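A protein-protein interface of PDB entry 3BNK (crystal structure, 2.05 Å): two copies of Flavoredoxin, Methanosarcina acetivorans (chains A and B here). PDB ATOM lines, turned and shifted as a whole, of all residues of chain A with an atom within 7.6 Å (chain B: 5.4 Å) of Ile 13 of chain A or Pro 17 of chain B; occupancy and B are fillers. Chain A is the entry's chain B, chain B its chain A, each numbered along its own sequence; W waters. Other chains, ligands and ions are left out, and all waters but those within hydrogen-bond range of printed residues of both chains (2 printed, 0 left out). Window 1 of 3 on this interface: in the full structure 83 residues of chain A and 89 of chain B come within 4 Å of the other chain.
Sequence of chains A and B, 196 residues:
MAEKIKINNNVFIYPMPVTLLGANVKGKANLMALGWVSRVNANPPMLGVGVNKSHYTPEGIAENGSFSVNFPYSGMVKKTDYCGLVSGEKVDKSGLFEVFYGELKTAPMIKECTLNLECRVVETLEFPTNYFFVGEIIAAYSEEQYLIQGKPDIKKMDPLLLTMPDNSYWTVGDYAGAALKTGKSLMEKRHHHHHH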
ATOM      1  N   VAL A  11      10.379 -25.466 -28.415  1.00  0.00           N
ATOM      2  CA  VAL A  11      11.422 -24.517 -28.758  1.00  0.00           C
ATOM      3  C   VAL A  11      11.446 -23.368 -27.765  1.00  0.00           C
ATOM      4  O   VAL A  11      10.400 -22.875 -27.308  1.00  0.00           O
ATOM      5  CB  VAL A  11      11.368 -24.076 -30.265  1.00  0.00           C
ATOM      6  CG1 VAL A  11      10.008 -24.345 -30.882  1.00  0.00           C
ATOM      7  CG2 VAL A  11      11.802 -22.627 -30.457  1.00  0.00           C
ATOM      8  N   PHE A  12      12.660 -22.965 -27.418  1.00  0.00           N
ATOM      9  CA  PHE A  12      12.875 -21.906 -26.459  1.00  0.00           C
ATOM     10  C   PHE A  12      13.083 -20.595 -27.210  1.00  0.00           C
ATOM     11  O   PHE A  12      13.235 -20.586 -28.441  1.00  0.00           O
ATOM     12  CB  PHE A  12      14.076 -22.257 -25.581  1.00  0.00           C
ATOM     13  CG  PHE A  12      13.807 -23.376 -24.596  1.00  0.00           C
ATOM     14  CD1 PHE A  12      13.854 -24.714 -24.996  1.00  0.00           C
ATOM     15  CD2 PHE A  12      13.514 -23.087 -23.265  1.00  0.00           C
ATOM     16  CE1 PHE A  12      13.617 -25.756 -24.085  1.00  0.00           C
ATOM     17  CE2 PHE A  12      13.272 -24.113 -22.339  1.00  0.00           C
ATOM     18  CZ  PHE A  12      13.317 -25.458 -22.754  1.00  0.00           C
ATOM     19  N   ILE A  13      13.068 -19.481 -26.480  1.00  0.00           N
ATOM     20  CA  ILE A  13      13.270 -18.184 -27.112  1.00  0.00           C
ATOM     21  C   ILE A  13      14.781 -18.038 -27.404  1.00  0.00           C
ATOM     22  O   ILE A  13      15.604 -18.425 -26.567  1.00  0.00           O
ATOM     23  CB  ILE A  13      12.748 -17.003 -26.220  1.00  0.00           C
ATOM     24  CG1 ILE A  13      11.305 -17.248 -25.760  1.00  0.00           C
ATOM     25  CG2 ILE A  13      12.897 -15.638 -26.947  1.00  0.00           C
ATOM     26  CD1 ILE A  13      10.295 -17.374 -26.887  1.00  0.00           C
ATOM     27  N   TYR A  14      15.105 -17.507 -28.584  1.00  0.00           N
ATOM     28  CA  TYR A  14      16.490 -17.289 -29.044  1.00  0.00           C
ATOM     29  C   TYR A  14      16.902 -15.813 -29.048  1.00  0.00           C
ATOM     30  O   TYR A  14      16.514 -15.071 -29.951  1.00  0.00           O
ATOM     31  CB  TYR A  14      16.708 -17.922 -30.437  1.00  0.00           C
ATOM     32  CG  TYR A  14      16.770 -19.430 -30.360  1.00  0.00           C
ATOM     33  CD1 TYR A  14      15.608 -20.190 -30.279  1.00  0.00           C
ATOM     34  CD2 TYR A  14      18.003 -20.096 -30.305  1.00  0.00           C
ATOM     35  CE1 TYR A  14      15.660 -21.589 -30.163  1.00  0.00           C
ATOM     36  CE2 TYR A  14      18.066 -21.486 -30.198  1.00  0.00           C
ATOM     37  CZ  TYR A  14      16.891 -22.224 -30.123  1.00  0.00           C
ATOM     38  OH  TYR A  14      16.960 -23.595 -29.997  1.00  0.00           O
ATOM     39  N   PRO A  15      17.679 -15.377 -28.029  1.00  0.00           N
ATOM     40  CA  PRO A  15      18.070 -16.131 -26.843  1.00  0.00           C
ATOM     41  C   PRO A  15      17.113 -15.816 -25.707  1.00  0.00           C
ATOM     42  O   PRO A  15      16.186 -15.020 -25.880  1.00  0.00           O
ATOM     43  CB  PRO A  15      19.424 -15.508 -26.489  1.00  0.00           C
ATOM     44  CG  PRO A  15      19.203 -14.034 -26.816  1.00  0.00           C
ATOM     45  CD  PRO A  15      18.277 -14.020 -28.016  1.00  0.00           C
ATOM     46  N   MET A  16      17.374 -16.431 -24.557  1.00  0.00           N
ATOM     47  CA  MET A  16      16.798 -16.039 -23.290  1.00  0.00           C
ATOM     48  C   MET A  16      17.733 -15.082 -22.559  1.00  0.00           C
ATOM     49  O   MET A  16      18.946 -15.103 -22.778  1.00  0.00           O
ATOM     50  CB  MET A  16      16.548 -17.263 -22.407  1.00  0.00           C
ATOM     51  CG  MET A  16      15.408 -18.154 -22.874  1.00  0.00           C
ATOM     52  SD  MET A  16      15.390 -19.726 -21.998  1.00  0.00           S
ATOM     53  CE  MET A  16      16.534 -20.667 -23.026  1.00  0.00           C
ATOM     54  N   PRO A  17      17.170 -14.256 -21.659  1.00  0.00           N
ATOM     55  CA  PRO A  17      17.997 -13.473 -20.750  1.00  0.00           C
ATOM     56  C   PRO A  17      18.522 -14.379 -19.623  1.00  0.00           C
ATOM     57  O   PRO A  17      18.078 -15.521 -19.484  1.00  0.00           O
ATOM     58  CB  PRO A  17      17.000 -12.456 -20.189  1.00  0.00           C
ATOM     59  CG  PRO A  17      15.695 -13.211 -20.188  1.00  0.00           C
ATOM     60  CD  PRO A  17      15.726 -14.044 -21.420  1.00  0.00           C
ATOM     61  N   GLY A  35      15.473 -17.794 -16.918  1.00  0.00           N
ATOM     62  CA  GLY A  35      15.537 -17.285 -18.290  1.00  0.00           C
ATOM     63  C   GLY A  35      14.154 -16.933 -18.794  1.00  0.00           C
ATOM     64  O   GLY A  35      14.013 -16.163 -19.748  1.00  0.00           O
ATOM     65  N   TRP A  36      13.123 -17.495 -18.152  1.00  0.00           N
ATOM     66  CA  TRP A  36      11.729 -17.224 -18.524  1.00  0.00           C
ATOM     67  C   TRP A  36      11.216 -15.976 -17.796  1.00  0.00           C
ATOM     68  O   TRP A  36      10.434 -16.085 -16.837  1.00  0.00           O
ATOM     69  CB  TRP A  36      10.822 -18.437 -18.227  1.00  0.00           C
ATOM     70  CG  TRP A  36      11.160 -19.715 -19.013  1.00  0.00           C
ATOM     71  CD1 TRP A  36      12.309 -19.975 -19.719  1.00  0.00           C
ATOM     72  CD2 TRP A  36      10.357 -20.898 -19.114  1.00  0.00           C
ATOM     73  NE1 TRP A  36      12.266 -21.233 -20.259  1.00  0.00           N
ATOM     74  CE2 TRP A  36      11.083 -21.830 -19.900  1.00  0.00           C
ATOM     75  CE3 TRP A  36       9.104 -21.272 -18.601  1.00  0.00           C
ATOM     76  CZ2 TRP A  36      10.582 -23.102 -20.213  1.00  0.00           C
ATOM     77  CZ3 TRP A  36       8.611 -22.541 -18.907  1.00  0.00           C
ATOM     78  CH2 TRP A  36       9.354 -23.442 -19.705  1.00  0.00           C
ATOM     79  N   VAL A  37      11.686 -14.810 -18.244  1.00  0.00           N
ATOM     80  CA  VAL A  37      11.260 -13.510 -17.712  1.00  0.00           C
ATOM     81  C   VAL A  37      10.907 -12.625 -18.876  1.00  0.00           C
ATOM     82  O   VAL A  37      11.653 -12.558 -19.852  1.00  0.00           O
ATOM     83  CB  VAL A  37      12.369 -12.651 -17.053  1.00  0.00           C
ATOM     84  CG1 VAL A  37      11.820 -11.921 -15.781  1.00  0.00           C
ATOM     85  CG2 VAL A  37      13.723 -13.387 -16.897  1.00  0.00           C
ATOM     86  N   SER A  38       9.821 -11.883 -18.736  1.00  0.00           N
ATOM     87  CA  SER A  38       9.430 -10.925 -19.740  1.00  0.00           C
ATOM     88  C   SER A  38       8.563  -9.850 -19.127  1.00  0.00           C
ATOM     89  O   SER A  38       7.891 -10.103 -18.140  1.00  0.00           O
ATOM     90  CB  SER A  38       8.624 -11.613 -20.838  1.00  0.00           C
ATOM     91  OG  SER A  38       8.153 -10.637 -21.713  1.00  0.00           O
ATOM     92  N   LEU A 162      21.177 -16.811 -22.794  1.00  0.00           N
ATOM     93  CA  LEU A 162      21.052 -18.243 -22.667  1.00  0.00           C
ATOM     94  C   LEU A 162      20.326 -18.812 -23.847  1.00  0.00           C
ATOM     95  O   LEU A 162      19.364 -18.237 -24.355  1.00  0.00           O
ATOM     96  CB  LEU A 162      20.334 -18.639 -21.369  1.00  0.00           C
ATOM     97  CG  LEU A 162      19.984 -20.131 -21.188  1.00  0.00           C
ATOM     98  CD1 LEU A 162      21.241 -20.958 -20.922  1.00  0.00           C
ATOM     99  CD2 LEU A 162      18.958 -20.341 -20.089  1.00  0.00           C
ATOM    100  N   THR A 163      20.791 -19.978 -24.252  1.00  0.00           N
ATOM    101  CA  THR A 163      20.156 -20.724 -25.295  1.00  0.00           C
ATOM    102  C   THR A 163      20.008 -22.190 -24.811  1.00  0.00           C
ATOM    103  O   THR A 163      20.941 -22.766 -24.257  1.00  0.00           O
ATOM    104  CB  THR A 163      20.949 -20.467 -26.616  1.00  0.00           C
ATOM    105  OG1 THR A 163      20.120 -20.669 -27.753  1.00  0.00           O
ATOM    106  CG2 THR A 163      22.190 -21.267 -26.702  1.00  0.00           C
ATOM    107  N   MET A 164      18.799 -22.741 -24.928  1.00  0.00           N
ATOM    108  CA  MET A 164      18.532 -24.148 -24.600  1.00  0.00           C
ATOM    109  C   MET A 164      17.849 -24.828 -25.803  1.00  0.00           C
ATOM    110  O   MET A 164      17.291 -24.134 -26.647  1.00  0.00           O
ATOM    111  CB  MET A 164      17.669 -24.254 -23.336  1.00  0.00           C
ATOM    112  CG  MET A 164      18.388 -23.847 -22.047  1.00  0.00           C
ATOM    113  SD  MET A 164      17.391 -24.093 -20.563  1.00  0.00           S
ATOM    114  CE  MET A 164      18.625 -24.082 -19.261  1.00  0.00           C
ATOM    115  N   PRO B  15      18.868  -8.005 -22.280  1.00  0.00           N
ATOM    116  CA  PRO B  15      18.085  -7.323 -23.318  1.00  0.00           C
ATOM    117  C   PRO B  15      16.765  -8.058 -23.540  1.00  0.00           C
ATOM    118  O   PRO B  15      16.491  -9.050 -22.865  1.00  0.00           O
ATOM    119  CB  PRO B  15      18.967  -7.468 -24.561  1.00  0.00           C
ATOM    120  CG  PRO B  15      19.697  -8.790 -24.339  1.00  0.00           C
ATOM    121  CD  PRO B  15      19.692  -9.093 -22.846  1.00  0.00           C
ATOM    122  N   MET B  16      15.965  -7.568 -24.481  1.00  0.00           N
ATOM    123  CA  MET B  16      14.762  -8.263 -24.917  1.00  0.00           C
ATOM    124  C   MET B  16      15.078  -9.066 -26.181  1.00  0.00           C
ATOM    125  O   MET B  16      16.011  -8.717 -26.928  1.00  0.00           O
ATOM    126  CB  MET B  16      13.648  -7.258 -25.222  1.00  0.00           C
ATOM    127  CG  MET B  16      12.856  -6.799 -23.988  1.00  0.00           C
ATOM    128  SD  MET B  16      11.875  -5.303 -24.278  1.00  0.00           S
ATOM    129  CE  MET B  16      11.074  -5.547 -25.832  1.00  0.00           C
ATOM    130  N   PRO B  17      14.283 -10.120 -26.452  1.00  0.00           N
ATOM    131  CA  PRO B  17      14.433 -10.754 -27.751  1.00  0.00           C
ATOM    132  C   PRO B  17      13.761  -9.858 -28.801  1.00  0.00           C
ATOM    133  O   PRO B  17      13.053  -8.905 -28.442  1.00  0.00           O
ATOM    134  CB  PRO B  17      13.651 -12.069 -27.590  1.00  0.00           C
ATOM    135  CG  PRO B  17      12.563 -11.727 -26.579  1.00  0.00           C
ATOM    136  CD  PRO B  17      13.220 -10.747 -25.632  1.00  0.00           C
ATOM    137  N   VAL B  18      14.012 -10.138 -30.075  1.00  0.00           N
ATOM    138  CA  VAL B  18      13.377  -9.401 -31.155  1.00  0.00           C
ATOM    139  C   VAL B  18      12.621 -10.361 -32.063  1.00  0.00           C
ATOM    140  O   VAL B  18      13.186 -11.241 -32.726  1.00  0.00           O
ATOM    141  CB  VAL B  18      14.365  -8.507 -31.960  1.00  0.00           C
ATOM    142  CG1 VAL B  18      13.663  -7.909 -33.184  1.00  0.00           C
ATOM    143  CG2 VAL B  18      14.870  -7.398 -31.084  1.00  0.00           C
ATOM    144  N   THR B  19      11.318 -10.165 -32.067  1.00  0.00           N
ATOM    145  CA  THR B  19      10.404 -11.093 -32.667  1.00  0.00           C
ATOM    146  C   THR B  19       9.384 -10.314 -33.503  1.00  0.00           C
ATOM    147  O   THR B  19       9.123  -9.132 -33.246  1.00  0.00           O
ATOM    148  CB  THR B  19       9.788 -11.928 -31.518  1.00  0.00           C
ATOM    149  OG1 THR B  19      10.449 -13.206 -31.419  1.00  0.00           O
ATOM    150  CG2 THR B  19       8.326 -12.037 -31.614  1.00  0.00           C
ATOM    151  N   LEU B  34       7.847  -7.375 -31.488  1.00  0.00           N
ATOM    152  CA  LEU B  34       7.496  -7.881 -30.182  1.00  0.00           C
ATOM    153  C   LEU B  34       8.712  -8.322 -29.373  1.00  0.00           C
ATOM    154  O   LEU B  34       9.404  -9.266 -29.742  1.00  0.00           O
ATOM    155  CB  LEU B  34       6.508  -9.054 -30.337  1.00  0.00           C
ATOM    156  CG  LEU B  34       6.030  -9.786 -29.086  1.00  0.00           C
ATOM    157  CD1 LEU B  34       4.840  -9.066 -28.436  1.00  0.00           C
ATOM    158  CD2 LEU B  34       5.654 -11.256 -29.447  1.00  0.00           C
ATOM    159  N   GLY B  35       8.945  -7.651 -28.253  1.00  0.00           N
ATOM    160  CA  GLY B  35       9.991  -8.061 -27.300  1.00  0.00           C
ATOM    161  C   GLY B  35       9.459  -8.692 -26.020  1.00  0.00           C
ATOM    162  O   GLY B  35      10.217  -9.230 -25.212  1.00  0.00           O
ATOM    163  N   VAL B  37       7.898 -11.466 -24.963  1.00  0.00           N
ATOM    164  CA  VAL B  37       7.554 -12.885 -25.130  1.00  0.00           C
ATOM    165  C   VAL B  37       8.458 -13.768 -24.277  1.00  0.00           C
ATOM    166  O   VAL B  37       9.671 -13.562 -24.210  1.00  0.00           O
ATOM    167  CB  VAL B  37       7.598 -13.343 -26.634  1.00  0.00           C
ATOM    168  CG1 VAL B  37       8.949 -13.023 -27.308  1.00  0.00           C
ATOM    169  CG2 VAL B  37       7.254 -14.843 -26.783  1.00  0.00           C
ATOM    170  N   SER B  38       7.865 -14.777 -23.659  1.00  0.00           N
ATOM    171  CA  SER B  38       8.596 -15.749 -22.878  1.00  0.00           C
ATOM    172  C   SER B  38       7.835 -17.057 -22.923  1.00  0.00           C
ATOM    173  O   SER B  38       6.589 -17.061 -23.025  1.00  0.00           O
ATOM    174  CB  SER B  38       8.723 -15.278 -21.419  1.00  0.00           C
ATOM    175  OG  SER B  38       9.185 -16.308 -20.558  1.00  0.00           O
ATOM    176  N   ARG B  39       8.582 -18.159 -22.836  1.00  0.00           N
ATOM    177  CA  ARG B  39       7.995 -19.456 -22.487  1.00  0.00           C
ATOM    178  C   ARG B  39       7.335 -19.348 -21.119  1.00  0.00           C
ATOM    179  O   ARG B  39       7.750 -18.559 -20.246  1.00  0.00           O
ATOM    180  CB  ARG B  39       9.019 -20.605 -22.522  1.00  0.00           C
ATOM    181  CG  ARG B  39       9.457 -21.040 -23.922  1.00  0.00           C
ATOM    182  CD  ARG B  39       8.353 -21.771 -24.715  1.00  0.00           C
ATOM    183  NE  ARG B  39       7.959 -22.993 -24.026  1.00  0.00           N
ATOM    184  CZ  ARG B  39       8.605 -24.147 -24.117  1.00  0.00           C
ATOM    185  NH1 ARG B  39       9.671 -24.263 -24.900  1.00  0.00           N
ATOM    186  NH2 ARG B  39       8.193 -25.182 -23.407  1.00  0.00           N
ATOM    187  N   LEU B  47       4.002 -20.430 -24.700  1.00  0.00           N
ATOM    188  CA  LEU B  47       4.654 -19.122 -24.569  1.00  0.00           C
ATOM    189  C   LEU B  47       3.574 -18.115 -24.221  1.00  0.00           C
ATOM    190  O   LEU B  47       2.403 -18.347 -24.503  1.00  0.00           O
ATOM    191  CB  LEU B  47       5.257 -18.647 -25.909  1.00  0.00           C
ATOM    192  CG  LEU B  47       6.286 -19.311 -26.813  1.00  0.00           C
ATOM    193  CD1 LEU B  47       6.160 -18.798 -28.264  1.00  0.00           C
ATOM    194  CD2 LEU B  47       7.673 -19.009 -26.301  1.00  0.00           C
ATOM    195  N   PHE B  71      11.251 -15.074 -35.875  1.00  0.00           N
ATOM    196  CA  PHE B  71      12.560 -14.528 -35.507  1.00  0.00           C
ATOM    197  C   PHE B  71      13.267 -14.005 -36.742  1.00  0.00           C
ATOM    198  O   PHE B  71      13.759 -14.787 -37.554  1.00  0.00           O
ATOM    199  CB  PHE B  71      13.438 -15.599 -34.821  1.00  0.00           C
ATOM    200  CG  PHE B  71      13.012 -15.938 -33.415  1.00  0.00           C
ATOM    201  CD1 PHE B  71      11.996 -16.869 -33.186  1.00  0.00           C
ATOM    202  CD2 PHE B  71      13.646 -15.346 -32.319  1.00  0.00           C
ATOM    203  CE1 PHE B  71      11.594 -17.185 -31.892  1.00  0.00           C
ATOM    204  CE2 PHE B  71      13.263 -15.645 -31.028  1.00  0.00           C
ATOM    205  CZ  PHE B  71      12.217 -16.585 -30.805  1.00  0.00           C
ATOM    206  N   LEU B 117       7.104 -19.892 -35.084  1.00  0.00           N
ATOM    207  CA  LEU B 117       6.333 -20.658 -34.102  1.00  0.00           C
ATOM    208  C   LEU B 117       4.847 -20.404 -34.289  1.00  0.00           C
ATOM    209  O   LEU B 117       4.393 -19.278 -34.143  1.00  0.00           O
ATOM    210  CB  LEU B 117       6.788 -20.339 -32.663  1.00  0.00           C
ATOM    211  CG  LEU B 117       8.304 -20.304 -32.403  1.00  0.00           C
ATOM    212  CD1 LEU B 117       8.598 -19.933 -30.982  1.00  0.00           C
ATOM    213  CD2 LEU B 117       9.000 -21.628 -32.762  1.00  0.00           C
ATOM    214  N   LEU B 160      18.171 -10.682 -33.534  1.00  0.00           N
ATOM    215  CA  LEU B 160      18.366  -9.352 -32.967  1.00  0.00           C
ATOM    216  C   LEU B 160      17.968  -9.340 -31.505  1.00  0.00           C
ATOM    217  O   LEU B 160      17.102 -10.097 -31.083  1.00  0.00           O
ATOM    218  CB  LEU B 160      17.565  -8.297 -33.757  1.00  0.00           C
ATOM    219  CG  LEU B 160      17.985  -8.045 -35.204  1.00  0.00           C
ATOM    220  CD1 LEU B 160      16.823  -7.544 -36.027  1.00  0.00           C
ATOM    221  CD2 LEU B 160      19.199  -7.058 -35.262  1.00  0.00           C
ATOM    222  N   LEU B 161      18.649  -8.494 -30.738  1.00  0.00           N
ATOM    223  CA  LEU B 161      18.341  -8.219 -29.336  1.00  0.00           C
ATOM    224  C   LEU B 161      17.917  -6.757 -29.223  1.00  0.00           C
ATOM    225  O   LEU B 161      18.247  -5.953 -30.096  1.00  0.00           O
ATOM    226  CB  LEU B 161      19.568  -8.476 -28.459  1.00  0.00           C
ATOM    227  CG  LEU B 161      20.369  -9.763 -28.707  1.00  0.00           C
ATOM    228  CD1 LEU B 161      21.587  -9.789 -27.815  1.00  0.00           C
ATOM    229  CD2 LEU B 161      19.473 -10.978 -28.438  1.00  0.00           C
ATOM    230  N   LEU B 162      17.209  -6.412 -28.155  1.00  0.00           N
ATOM    231  CA  LEU B 162      16.669  -5.067 -28.014  1.00  0.00           C
ATOM    232  C   LEU B 162      16.796  -4.537 -26.595  1.00  0.00           C
ATOM    233  O   LEU B 162      16.547  -5.232 -25.611  1.00  0.00           O
ATOM    234  CB  LEU B 162      15.191  -4.977 -28.484  1.00  0.00           C
ATOM    235  CG  LEU B 162      14.410  -3.684 -28.147  1.00  0.00           C
ATOM    236  CD1 LEU B 162      14.770  -2.558 -29.138  1.00  0.00           C
ATOM    237  CD2 LEU B 162      12.913  -3.890 -28.122  1.00  0.00           C
HETATM  238  O   HOH W   1      10.792  -8.733 -22.379  1.00  0.00           O
HETATM  239  O   HOH W   2      15.790 -12.611 -30.479  1.00  0.00           O
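Water W2 lies within hydrogen-bond range of the backbone carbonyl oxygen of Tyr 14 of chain A (2.6 Å), the backbone carbonyl oxygen of Leu 160 of chain B (2.9 Å) and the backbone NH of Val 18 of chain B (3.1 Å). Water W1 bridges O of Gly 35 of chain B (2.9 Å) and OG of Ser 38 of chain A (3.3 Å).
Ile 13 of chain A touches just these residues of chain B: Pro 17 (3.7 Å), Val 37 (3.96 Å) and Leu 47 (3.1 Å). Gly 35 of chain A touches none of the printed residues of chain B. Of the printed residues of chain B, Trp 36 of chain A touches Ser 38 (3.4 Å) and Arg 39 (3.4 Å). Leu 162 of chain A touches none of the printed residues of chain B. Pro 17 of chain B touches one residue of chain A. Printed residues of chain A within 4 Å of Val 37 of chain B: Ile 13 and Ser 38. Printed residues of chain A within 4 Å of Arg 39 of chain B: Val 11 (2.9 Å) and Trp 36 (3.4 Å). Printed residues of chain A within 4 Å of Leu 161 of chain B: Pro 15 (3.3 Å). The nearest residue of chain B that does not touch Ile 13 of chain A is Phe 71 of chain B (4.03 Å). The nearest residue of chain A that does not touch Pro 17 of chain B is Pro 15 of chain A (4.2 Å). The nearest printed residue of chain B that does not touch Pro 15 of chain A is Pro 17 of chain B (4.2 Å).
O of Val 11 of chain A is in hydrogen-bond range of NH1 of Arg 39 of chain B. The backbone NH (N) of Val 37 of chain B lies within hydrogen-bond range of the side-chain hydroxyl (OG) of Ser 38 of chain A (3.4 Å).
Hydrophobic or aromatic side chains of chain A within 4 Å of the printed part of chain B: Val 11, Ile 13, Pro 15 and Trp 36. Printed residues of chain B that touch a printed residue of chain A: Pro 17, Val 37, Ser 38, Arg 39, Leu 47, Phe 71, Leu 117 and Leu 161. Among the printed residues, 12 pairs touch across the chains. Among the printed residues, no Asp or Glu carboxylate lies within 4 Å of a Lys or Arg side-chain nitrogen of the other chain.
CG1 of Val 11 of chain A touches CD2 of Leu 117 of chain B, at 3.5 Å. Ile 13 of chain A touches Pro 17 of chain B. Val 37 of chain B touches Ile 13 of chain A. CD1 of Ile 13 of chain A touches CD2 of Leu 47 of chain B, at 3.1 Å. O of Tyr 14 of chain A touches CE2 of Phe 71 of chain B, 3.5 Å away. CD2 of Leu 161 of chain B touches CD of Pro 15 of chain A (3.3 Å). OG of Ser 38 of chain B touches CA of Trp 36 of chain A (3.4 Å). Arg 39 of chain B touches Trp 36 of chain A. N of Val 37 of chain A touches OG of Ser 38 of chain B, 3.7 Å away. Ser 38 of chain B touches Ser 38 of chain A (CB to CB, 3.7 Å).
The backbone carbonyl oxygen of Met 164 of chain A sits at hydrogen-bond distance from the side-chain hydroxyl of Tyr 14 of chain A, at 3.4 Å.
Val 37 of chain A touches Ser 38 of chain B, and with the chains exchanged Ser 38 of chain A touches Val 37 of chain B. Ser 38 of chain A touches its own counterpart, Ser 38 of chain B. Positions printed for both chains: 15, 16, 17, 35, 37, 38 and 162. Of the 12 pairs that touch across the chains among the printed residues, 3 have their exchanged pair printed and touching as well.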
